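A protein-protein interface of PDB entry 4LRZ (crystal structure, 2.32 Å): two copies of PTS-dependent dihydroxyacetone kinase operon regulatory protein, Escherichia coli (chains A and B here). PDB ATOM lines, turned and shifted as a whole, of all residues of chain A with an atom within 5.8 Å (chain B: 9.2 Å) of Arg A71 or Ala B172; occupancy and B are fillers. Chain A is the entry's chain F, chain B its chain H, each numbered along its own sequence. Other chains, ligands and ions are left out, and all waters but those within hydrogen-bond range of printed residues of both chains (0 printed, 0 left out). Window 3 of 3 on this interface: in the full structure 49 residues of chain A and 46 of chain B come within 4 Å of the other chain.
OG1 of Thr A171 lies within hydrogen-bond range of OG1 of Thr B171, 3.2 Å away.
The backbone carbonyl oxygen (O) of Gln A169 lies within hydrogen-bond range of the guanidinium group (NH2) of Arg A71 (3.3 Å). O of Leu B175 sits at hydrogen-bond distance from OG1 of Thr B178 (3.0 Å). The side-chain sulfur (SG) of Cys B146 is in hydrogen-bond range of the backbone NH (N) of Leu B175 (3.7 Å). The guanidinium group of Arg A71 lies within salt-bridge range of the side-chain carboxylate of Asp A174 (2.8 Å). The side-chain hydroxyl of Thr B171 lies within hydrogen-bond range of the side-chain carboxylate of Asp B174 (2.8 Å). The backbone NH of Ala B173 lies close to the side-chain hydroxyl of Thr B171, at 3.4 Å.
Among the printed residues, pairs that only touch across the chains: Tyr A67 with Leu B175, Tyr A67 with Pro B176, Met A68 with Ala B172, Met A68 with Ala B173, Met A68 with Pro B176, Arg A71 with Ala B172, Thr A171 with Ala B173 and Asp A174 with Ala B173.
Of the printed residues of chain B, Arg A71 touches Ala B172. Of chain B, only Ala B172, Ala B173 and Pro B176 come within 4 Å of Met A68. No residue of chain B comes within 4 Å of Pro A70. Printed residues of chain A within 4 Å of Pro B176: Tyr A67 and Met A68. Printed residues of chain A within 4 Å of Leu B175: Tyr A67. Printed residues of chain B within 4 Å of Asp A174: Ala B173 (3.5 Å). Of the printed residues of chain A, Thr B171 touches Thr A171. Of the printed residues of chain B, Thr A171 touches Thr B171 and Ala B173. Thr B170 touches none of the printed residues of chain A. The nearest residue of chain B that does not touch Arg A71 is Ala B173 (4.2 Å). The nearest residue of chain A that does not touch Ala B172 is Tyr A67 (4.1 Å).
Hydrophobic or aromatic side chains of chain B that line the printed part of chain A: Ala B172, Ala B173, Leu B175 and Pro B176. Hydrophobic or aromatic side chains of chain A that line the printed part of chain B: Tyr A67 and Met A68. Along chain A the printed residues that touch a printed residue of chain B span positions 67 to 174. Among the printed residues, 9 pairs touch across the chains. Among the printed residues, no Asp or Glu carboxylate lies within 4 Å of a Lys or Arg side-chain nitrogen of the other chain.
Thr B171 touches its own counterpart, Thr A171. Of the 9 pairs that touch across the chains among the printed residues, 1 has its exchanged pair printed and touching as well.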
ATOM      1  N   TRP A  65      -5.650  11.855   4.779  1.00  0.00           N
ATOM      2  CA  TRP A  65      -4.532  10.994   5.186  1.00  0.00           C
ATOM      3  C   TRP A  65      -4.094  11.278   6.633  1.00  0.00           C
ATOM      4  O   TRP A  65      -3.993  10.365   7.455  1.00  0.00           O
ATOM      5  CB  TRP A  65      -3.350  11.136   4.207  1.00  0.00           C
ATOM      6  CG  TRP A  65      -2.164  10.358   4.614  1.00  0.00           C
ATOM      7  CD1 TRP A  65      -0.900  10.827   4.787  1.00  0.00           C
ATOM      8  CD2 TRP A  65      -2.132   8.961   4.942  1.00  0.00           C
ATOM      9  NE1 TRP A  65      -0.078   9.808   5.201  1.00  0.00           N
ATOM     10  CE2 TRP A  65      -0.807   8.650   5.295  1.00  0.00           C
ATOM     11  CE3 TRP A  65      -3.099   7.946   4.965  1.00  0.00           C
ATOM     12  CZ2 TRP A  65      -0.412   7.354   5.688  1.00  0.00           C
ATOM     13  CZ3 TRP A  65      -2.716   6.672   5.363  1.00  0.00           C
ATOM     14  CH2 TRP A  65      -1.377   6.387   5.726  1.00  0.00           C
ATOM     15  N   TYR A  67      -5.591  12.434   9.276  1.00  0.00           N
ATOM     16  CA  TYR A  67      -6.473  11.911  10.331  1.00  0.00           C
ATOM     17  C   TYR A  67      -6.724  10.402  10.294  1.00  0.00           C
ATOM     18  O   TYR A  67      -7.425   9.871  11.159  1.00  0.00           O
ATOM     19  CB  TYR A  67      -7.793  12.680  10.388  1.00  0.00           C
ATOM     20  CG  TYR A  67      -7.561  14.074  10.828  1.00  0.00           C
ATOM     21  CD1 TYR A  67      -7.546  14.409  12.183  1.00  0.00           C
ATOM     22  CD2 TYR A  67      -7.265  15.056   9.893  1.00  0.00           C
ATOM     23  CE1 TYR A  67      -7.286  15.688  12.581  1.00  0.00           C
ATOM     24  CE2 TYR A  67      -7.019  16.331  10.278  1.00  0.00           C
ATOM     25  CZ  TYR A  67      -7.027  16.647  11.616  1.00  0.00           C
ATOM     26  OH  TYR A  67      -6.760  17.940  11.947  1.00  0.00           O
ATOM     27  N   MET A  68      -6.094   9.740   9.326  1.00  0.00           N
ATOM     28  CA  MET A  68      -6.174   8.312   9.128  1.00  0.00           C
ATOM     29  C   MET A  68      -4.876   7.544   9.420  1.00  0.00           C
ATOM     30  O   MET A  68      -4.927   6.356   9.786  1.00  0.00           O
ATOM     31  CB  MET A  68      -6.547   8.051   7.668  1.00  0.00           C
ATOM     32  CG  MET A  68      -7.296   6.781   7.460  1.00  0.00           C
ATOM     33  SD  MET A  68      -7.870   6.758   5.787  1.00  0.00           S
ATOM     34  CE  MET A  68      -9.468   6.118   6.114  1.00  0.00           C
ATOM     35  N   ALA A  69      -3.724   8.166   9.168  1.00  0.00           N
ATOM     36  CA  ALA A  69      -2.424   7.526   9.419  1.00  0.00           C
ATOM     37  C   ALA A  69      -2.333   7.119  10.907  1.00  0.00           C
ATOM     38  O   ALA A  69      -2.700   7.937  11.778  1.00  0.00           O
ATOM     39  CB  ALA A  69      -1.272   8.491   9.048  1.00  0.00           C
ATOM     40  N   PRO A  70      -1.846   5.892  11.225  1.00  0.00           N
ATOM     41  CA  PRO A  70      -1.241   4.814  10.422  1.00  0.00           C
ATOM     42  C   PRO A  70      -2.264   3.811   9.886  1.00  0.00           C
ATOM     43  O   PRO A  70      -3.220   3.447  10.593  1.00  0.00           O
ATOM     44  CB  PRO A  70      -0.317   4.102  11.414  1.00  0.00           C
ATOM     45  CG  PRO A  70      -0.888   4.465  12.833  1.00  0.00           C
ATOM     46  CD  PRO A  70      -1.982   5.493  12.645  1.00  0.00           C
ATOM     47  N   ARG A  71      -2.036   3.373   8.649  1.00  0.00           N
ATOM     48  CA  ARG A  71      -2.965   2.568   7.898  1.00  0.00           C
ATOM     49  C   ARG A  71      -2.284   2.190   6.569  1.00  0.00           C
ATOM     50  O   ARG A  71      -1.612   3.019   5.969  1.00  0.00           O
ATOM     51  CB  ARG A  71      -4.241   3.369   7.651  1.00  0.00           C
ATOM     52  CG  ARG A  71      -5.026   2.884   6.495  1.00  0.00           C
ATOM     53  CD  ARG A  71      -6.525   3.116   6.578  1.00  0.00           C
ATOM     54  NE  ARG A  71      -7.177   1.973   5.918  1.00  0.00           N
ATOM     55  CZ  ARG A  71      -8.332   2.002   5.276  1.00  0.00           C
ATOM     56  NH1 ARG A  71      -9.023   3.142   5.149  1.00  0.00           N
ATOM     57  NH2 ARG A  71      -8.798   0.884   4.760  1.00  0.00           N
ATOM     58  N   GLU A  72      -2.415   0.945   6.131  1.00  0.00           N
ATOM     59  CA  GLU A  72      -1.897   0.532   4.806  1.00  0.00           C
ATOM     60  C   GLU A  72      -2.893   0.896   3.708  1.00  0.00           C
ATOM     61  O   GLU A  72      -3.772   0.099   3.377  1.00  0.00           O
ATOM     62  CB  GLU A  72      -1.611  -0.977   4.768  1.00  0.00           C
ATOM     63  CG  GLU A  72      -0.358  -1.447   5.556  1.00  0.00           C
ATOM     64  CD  GLU A  72      -0.271  -2.977   5.713  1.00  0.00           C
ATOM     65  OE1 GLU A  72      -0.435  -3.454   6.863  1.00  0.00           O
ATOM     66  OE2 GLU A  72      -0.040  -3.713   4.711  1.00  0.00           O
ATOM     67  N   CYS A  73      -2.788   2.109   3.168  1.00  0.00           N
ATOM     68  CA  CYS A  73      -3.691   2.519   2.123  1.00  0.00           C
ATOM     69  C   CYS A  73      -3.119   3.666   1.303  1.00  0.00           C
ATOM     70  O   CYS A  73      -2.130   4.266   1.671  1.00  0.00           O
ATOM     71  CB  CYS A  73      -5.072   2.901   2.672  1.00  0.00           C
ATOM     72  SG  CYS A  73      -5.150   4.573   3.321  1.00  0.00           S
ATOM     73  N   ASP A  90       0.160   5.915   2.496  1.00  0.00           N
ATOM     74  CA  ASP A  90       1.248   5.183   3.100  1.00  0.00           C
ATOM     75  C   ASP A  90       2.339   4.813   2.088  1.00  0.00           C
ATOM     76  O   ASP A  90       2.057   4.161   1.078  1.00  0.00           O
ATOM     77  CB  ASP A  90       0.707   3.929   3.782  1.00  0.00           C
ATOM     78  CG  ASP A  90       1.799   2.984   4.189  1.00  0.00           C
ATOM     79  OD1 ASP A  90       2.582   3.328   5.085  1.00  0.00           O
ATOM     80  OD2 ASP A  90       1.875   1.885   3.621  1.00  0.00           O
ATOM     81  N   THR A  93       2.479   1.240   0.781  1.00  0.00           N
ATOM     82  CA  THR A  93       1.339   0.867  -0.025  1.00  0.00           C
ATOM     83  C   THR A  93       1.537   1.494  -1.412  1.00  0.00           C
ATOM     84  O   THR A  93       1.368   0.833  -2.420  1.00  0.00           O
ATOM     85  CB  THR A  93       0.023   1.218   0.692  1.00  0.00           C
ATOM     86  OG1 THR A  93       0.034   0.608   1.990  1.00  0.00           O
ATOM     87  CG2 THR A  93      -1.172   0.717  -0.039  1.00  0.00           C
ATOM     88  N   LEU A 163      -9.553   5.340  -3.029  1.00  0.00           N
ATOM     89  CA  LEU A 163      -8.823   4.819  -1.914  1.00  0.00           C
ATOM     90  C   LEU A 163      -8.520   3.339  -2.202  1.00  0.00           C
ATOM     91  O   LEU A 163      -9.433   2.550  -2.432  1.00  0.00           O
ATOM     92  CB  LEU A 163      -9.681   4.941  -0.662  1.00  0.00           C
ATOM     93  CG  LEU A 163      -9.177   4.436   0.696  1.00  0.00           C
ATOM     94  CD1 LEU A 163      -9.776   5.303   1.818  1.00  0.00           C
ATOM     95  CD2 LEU A 163      -9.461   2.963   0.927  1.00  0.00           C
ATOM     96  N   CYS A 165      -6.454  -0.216  -0.859  1.00  0.00           N
ATOM     97  CA  CYS A 165      -5.896  -0.906   0.301  1.00  0.00           C
ATOM     98  C   CYS A 165      -5.900  -2.412   0.148  1.00  0.00           C
ATOM     99  O   CYS A 165      -6.759  -2.942  -0.554  1.00  0.00           O
ATOM    100  CB  CYS A 165      -6.630  -0.519   1.603  1.00  0.00           C
ATOM    101  SG  CYS A 165      -8.299  -1.166   1.858  1.00  0.00           S
ATOM    102  N   GLN A 169      -7.739  -5.483   4.843  1.00  0.00           N
ATOM    103  CA  GLN A 169      -7.826  -4.314   5.720  1.00  0.00           C
ATOM    104  C   GLN A 169      -8.902  -3.288   5.364  1.00  0.00           C
ATOM    105  O   GLN A 169      -8.910  -2.189   5.909  1.00  0.00           O
ATOM    106  CB  GLN A 169      -6.491  -3.605   5.752  1.00  0.00           C
ATOM    107  CG  GLN A 169      -5.378  -4.424   6.318  1.00  0.00           C
ATOM    108  CD  GLN A 169      -4.078  -3.714   6.155  1.00  0.00           C
ATOM    109  OE1 GLN A 169      -3.938  -2.540   6.536  1.00  0.00           O
ATOM    110  NE2 GLN A 169      -3.109  -4.398   5.562  1.00  0.00           N
ATOM    111  N   THR A 170      -9.799  -3.636   4.455  1.00  0.00           N
ATOM    112  CA  THR A 170     -10.836  -2.708   4.041  1.00  0.00           C
ATOM    113  C   THR A 170     -11.671  -2.295   5.252  1.00  0.00           C
ATOM    114  O   THR A 170     -11.821  -3.075   6.159  1.00  0.00           O
ATOM    115  CB  THR A 170     -11.703  -3.298   2.902  1.00  0.00           C
ATOM    116  OG1 THR A 170     -12.470  -2.241   2.304  1.00  0.00           O
ATOM    117  CG2 THR A 170     -12.626  -4.412   3.413  1.00  0.00           C
ATOM    118  N   THR A 171     -12.164  -1.064   5.307  1.00  0.00           N
ATOM    119  CA  THR A 171     -13.132  -0.725   6.369  1.00  0.00           C
ATOM    120  C   THR A 171     -14.436  -0.226   5.763  1.00  0.00           C
ATOM    121  O   THR A 171     -14.457   0.249   4.630  1.00  0.00           O
ATOM    122  CB  THR A 171     -12.611   0.313   7.439  1.00  0.00           C
ATOM    123  OG1 THR A 171     -12.788   1.650   6.970  1.00  0.00           O
ATOM    124  CG2 THR A 171     -11.152   0.110   7.768  1.00  0.00           C
ATOM    125  N   ASP A 174     -14.560   3.456   4.283  1.00  0.00           N
ATOM    126  CA  ASP A 174     -13.759   3.797   3.107  1.00  0.00           C
ATOM    127  C   ASP A 174     -14.573   4.408   1.967  1.00  0.00           C
ATOM    128  O   ASP A 174     -14.205   5.450   1.403  1.00  0.00           O
ATOM    129  CB  ASP A 174     -12.982   2.569   2.636  1.00  0.00           C
ATOM    130  CG  ASP A 174     -11.926   2.102   3.676  1.00  0.00           C
ATOM    131  OD1 ASP A 174     -11.769   2.775   4.725  1.00  0.00           O
ATOM    132  OD2 ASP A 174     -11.258   1.057   3.467  1.00  0.00           O
ATOM    133  N   MET B  68     -22.285   3.057   3.791  1.00  0.00           N
ATOM    134  CA  MET B  68     -21.589   2.433   4.920  1.00  0.00           C
ATOM    135  C   MET B  68     -22.328   1.218   5.512  1.00  0.00           C
ATOM    136  O   MET B  68     -21.709   0.330   6.089  1.00  0.00           O
ATOM    137  CB  MET B  68     -21.353   3.506   6.001  1.00  0.00           C
ATOM    138  CG  MET B  68     -20.888   3.059   7.353  1.00  0.00           C
ATOM    139  SD  MET B  68     -20.197   4.455   8.277  1.00  0.00           S
ATOM    140  CE  MET B  68     -18.563   4.168   7.714  1.00  0.00           C
ATOM    141  N   ARG B  71     -23.453  -1.906   9.584  1.00  0.00           N
ATOM    142  CA  ARG B  71     -22.361  -1.678  10.525  1.00  0.00           C
ATOM    143  C   ARG B  71     -22.993  -1.176  11.826  1.00  0.00           C
ATOM    144  O   ARG B  71     -23.990  -0.476  11.772  1.00  0.00           O
ATOM    145  CB  ARG B  71     -21.414  -0.625   9.946  1.00  0.00           C
ATOM    146  CG  ARG B  71     -20.759   0.207  10.951  1.00  0.00           C
ATOM    147  CD  ARG B  71     -19.690   1.148  10.461  1.00  0.00           C
ATOM    148  NE  ARG B  71     -18.725   1.310  11.561  1.00  0.00           N
ATOM    149  CZ  ARG B  71     -17.840   2.286  11.681  1.00  0.00           C
ATOM    150  NH1 ARG B  71     -17.792   3.254  10.751  1.00  0.00           N
ATOM    151  NH2 ARG B  71     -17.003   2.290  12.730  1.00  0.00           N
ATOM    152  N   LYS B 129     -10.996  12.203  18.184  1.00  0.00           N
ATOM    153  CA  LYS B 129     -11.514  10.861  18.460  1.00  0.00           C
ATOM    154  C   LYS B 129     -11.189  10.481  19.911  1.00  0.00           C
ATOM    155  O   LYS B 129     -10.051  10.658  20.351  1.00  0.00           O
ATOM    156  CB  LYS B 129     -10.795   9.849  17.575  1.00  0.00           C
ATOM    157  CG  LYS B 129     -11.331   8.415  17.684  1.00  0.00           C
ATOM    158  CD  LYS B 129     -10.499   7.470  16.777  1.00  0.00           C
ATOM    159  CE  LYS B 129     -11.274   6.243  16.398  1.00  0.00           C
ATOM    160  NZ  LYS B 129     -10.363   5.248  15.763  1.00  0.00           N
ATOM    161  N   MET B 131     -11.648   7.165  22.793  1.00  0.00           N
ATOM    162  CA  MET B 131     -12.014   5.751  22.828  1.00  0.00           C
ATOM    163  C   MET B 131     -11.843   5.199  24.198  1.00  0.00           C
ATOM    164  O   MET B 131     -10.897   5.585  24.884  1.00  0.00           O
ATOM    165  CB  MET B 131     -11.070   4.920  21.928  1.00  0.00           C
ATOM    166  CG  MET B 131     -11.041   5.295  20.476  1.00  0.00           C
ATOM    167  SD  MET B 131      -9.755   4.348  19.571  1.00  0.00           S
ATOM    168  CE  MET B 131      -9.996   2.676  20.194  1.00  0.00           C
ATOM    169  N   CYS B 146     -16.054   9.930  17.266  1.00  0.00           N
ATOM    170  CA  CYS B 146     -15.219  10.752  16.412  1.00  0.00           C
ATOM    171  C   CYS B 146     -16.044  11.979  16.245  1.00  0.00           C
ATOM    172  O   CYS B 146     -17.254  11.855  16.170  1.00  0.00           O
ATOM    173  CB  CYS B 146     -15.025  10.110  15.034  1.00  0.00           C
ATOM    174  SG  CYS B 146     -13.847   8.747  15.048  1.00  0.00           S
ATOM    175  N   LEU B 163     -19.693  10.520  14.982  1.00  0.00           N
ATOM    176  CA  LEU B 163     -19.881   9.124  14.686  1.00  0.00           C
ATOM    177  C   LEU B 163     -19.565   8.341  15.956  1.00  0.00           C
ATOM    178  O   LEU B 163     -18.502   8.531  16.578  1.00  0.00           O
ATOM    179  CB  LEU B 163     -18.885   8.715  13.593  1.00  0.00           C
ATOM    180  CG  LEU B 163     -18.943   7.307  13.006  1.00  0.00           C
ATOM    181  CD1 LEU B 163     -18.558   7.364  11.489  1.00  0.00           C
ATOM    182  CD2 LEU B 163     -18.078   6.271  13.810  1.00  0.00           C
ATOM    183  N   CYS B 165     -19.538   4.353  17.693  1.00  0.00           N
ATOM    184  CA  CYS B 165     -19.598   2.940  17.493  1.00  0.00           C
ATOM    185  C   CYS B 165     -18.998   2.191  18.690  1.00  0.00           C
ATOM    186  O   CYS B 165     -18.194   2.772  19.409  1.00  0.00           O
ATOM    187  CB  CYS B 165     -18.848   2.577  16.192  1.00  0.00           C
ATOM    188  SG  CYS B 165     -17.079   2.772  16.340  1.00  0.00           S
ATOM    189  N   GLN B 169     -15.216  -1.970  17.341  1.00  0.00           N
ATOM    190  CA  GLN B 169     -15.478  -1.873  15.907  1.00  0.00           C
ATOM    191  C   GLN B 169     -14.965  -0.603  15.228  1.00  0.00           C
ATOM    192  O   GLN B 169     -15.301  -0.348  14.098  1.00  0.00           O
ATOM    193  CB  GLN B 169     -16.962  -2.034  15.644  1.00  0.00           C
ATOM    194  CG  GLN B 169     -17.531  -3.312  16.272  1.00  0.00           C
ATOM    195  CD  GLN B 169     -18.914  -3.619  15.758  1.00  0.00           C
ATOM    196  OE1 GLN B 169     -19.362  -3.046  14.747  1.00  0.00           O
ATOM    197  NE2 GLN B 169     -19.613  -4.524  16.446  1.00  0.00           N
ATOM    198  N   THR B 170     -14.150   0.199  15.912  1.00  0.00           N
ATOM    199  CA  THR B 170     -13.748   1.478  15.333  1.00  0.00           C
ATOM    200  C   THR B 170     -12.865   1.276  14.115  1.00  0.00           C
ATOM    201  O   THR B 170     -12.130   0.289  14.057  1.00  0.00           O
ATOM    202  CB  THR B 170     -13.037   2.401  16.344  1.00  0.00           C
ATOM    203  OG1 THR B 170     -13.025   3.725  15.789  1.00  0.00           O
ATOM    204  CG2 THR B 170     -11.609   1.939  16.604  1.00  0.00           C
ATOM    205  N   THR B 171     -12.927   2.210  13.158  1.00  0.00           N
ATOM    206  CA  THR B 171     -12.081   2.116  11.949  1.00  0.00           C
ATOM    207  C   THR B 171     -11.271   3.390  11.717  1.00  0.00           C
ATOM    208  O   THR B 171     -11.686   4.485  12.105  1.00  0.00           O
ATOM    209  CB  THR B 171     -12.854   1.680  10.623  1.00  0.00           C
ATOM    210  OG1 THR B 171     -13.293   2.810   9.868  1.00  0.00           O
ATOM    211  CG2 THR B 171     -14.050   0.816  10.912  1.00  0.00           C
ATOM    212  N   ALA B 172     -10.123   3.228  11.079  1.00  0.00           N
ATOM    213  CA  ALA B 172      -9.206   4.315  10.757  1.00  0.00           C
ATOM    214  C   ALA B 172      -9.874   5.428   9.929  1.00  0.00           C
ATOM    215  O   ALA B 172      -9.454   6.576   9.952  1.00  0.00           O
ATOM    216  CB  ALA B 172      -7.963   3.741   9.985  1.00  0.00           C
ATOM    217  N   ALA B 173     -10.901   5.076   9.189  1.00  0.00           N
ATOM    218  CA  ALA B 173     -11.560   6.028   8.334  1.00  0.00           C
ATOM    219  C   ALA B 173     -12.658   6.847   9.013  1.00  0.00           C
ATOM    220  O   ALA B 173     -13.142   7.794   8.442  1.00  0.00           O
ATOM    221  CB  ALA B 173     -12.124   5.303   7.078  1.00  0.00           C
ATOM    222  N   ASP B 174     -13.066   6.474  10.219  1.00  0.00           N
ATOM    223  CA  ASP B 174     -14.203   7.156  10.889  1.00  0.00           C
ATOM    224  C   ASP B 174     -13.945   8.628  11.112  1.00  0.00           C
ATOM    225  O   ASP B 174     -14.849   9.436  10.961  1.00  0.00           O
ATOM    226  CB  ASP B 174     -14.535   6.479  12.236  1.00  0.00           C
ATOM    227  CG  ASP B 174     -14.912   4.998  12.066  1.00  0.00           C
ATOM    228  OD1 ASP B 174     -15.166   4.579  10.921  1.00  0.00           O
ATOM    229  OD2 ASP B 174     -14.975   4.258  13.067  1.00  0.00           O
ATOM    230  N   LEU B 175     -12.732   8.984  11.490  1.00  0.00           N
ATOM    231  CA  LEU B 175     -12.439  10.358  11.860  1.00  0.00           C
ATOM    232  C   LEU B 175     -12.374  11.248  10.620  1.00  0.00           C
ATOM    233  O   LEU B 175     -13.144  12.231  10.540  1.00  0.00           O
ATOM    234  CB  LEU B 175     -11.149  10.450  12.702  1.00  0.00           C
ATOM    235  CG  LEU B 175     -10.709  11.813  13.267  1.00  0.00           C
ATOM    236  CD1 LEU B 175     -11.672  12.399  14.340  1.00  0.00           C
ATOM    237  CD2 LEU B 175      -9.295  11.647  13.875  1.00  0.00           C
ATOM    238  N   PRO B 176     -11.511  10.890   9.626  1.00  0.00           N
ATOM    239  CA  PRO B 176     -11.517  11.672   8.378  1.00  0.00           C
ATOM    240  C   PRO B 176     -12.899  11.779   7.756  1.00  0.00           C
ATOM    241  O   PRO B 176     -13.180  12.748   7.101  1.00  0.00           O
ATOM    242  CB  PRO B 176     -10.506  10.940   7.464  1.00  0.00           C
ATOM    243  CG  PRO B 176     -10.169   9.620   8.118  1.00  0.00           C
ATOM    244  CD  PRO B 176     -10.450   9.858   9.620  1.00  0.00           C
ATOM    245  N   LEU B 177     -13.785  10.817   8.004  1.00  0.00           N
ATOM    246  CA  LEU B 177     -15.164  10.892   7.491  1.00  0.00           C
ATOM    247  C   LEU B 177     -15.957  12.023   8.110  1.00  0.00           C
ATOM    248  O   LEU B 177     -16.662  12.762   7.387  1.00  0.00           O
ATOM    249  CB  LEU B 177     -15.895   9.556   7.673  1.00  0.00           C
ATOM    250  CG  LEU B 177     -17.329   9.434   7.144  1.00  0.00           C
ATOM    251  CD1 LEU B 177     -17.469   9.661   5.612  1.00  0.00           C
ATOM    252  CD2 LEU B 177     -17.910   8.087   7.536  1.00  0.00           C
ATOM    253  N   THR B 178     -15.856  12.190   9.445  1.00  0.00           N
ATOM    254  CA  THR B 178     -16.657  13.215  10.126  1.00  0.00           C
ATOM    255  C   THR B 178     -16.086  14.553   9.642  1.00  0.00           C
ATOM    256  O   THR B 178     -16.819  15.478   9.371  1.00  0.00           O
ATOM    257  CB  THR B 178     -16.662  13.085  11.691  1.00  0.00           C
ATOM    258  OG1 THR B 178     -15.360  13.326  12.212  1.00  0.00           O
ATOM    259  CG2 THR B 178     -17.089  11.742  12.148  1.00  0.00           C
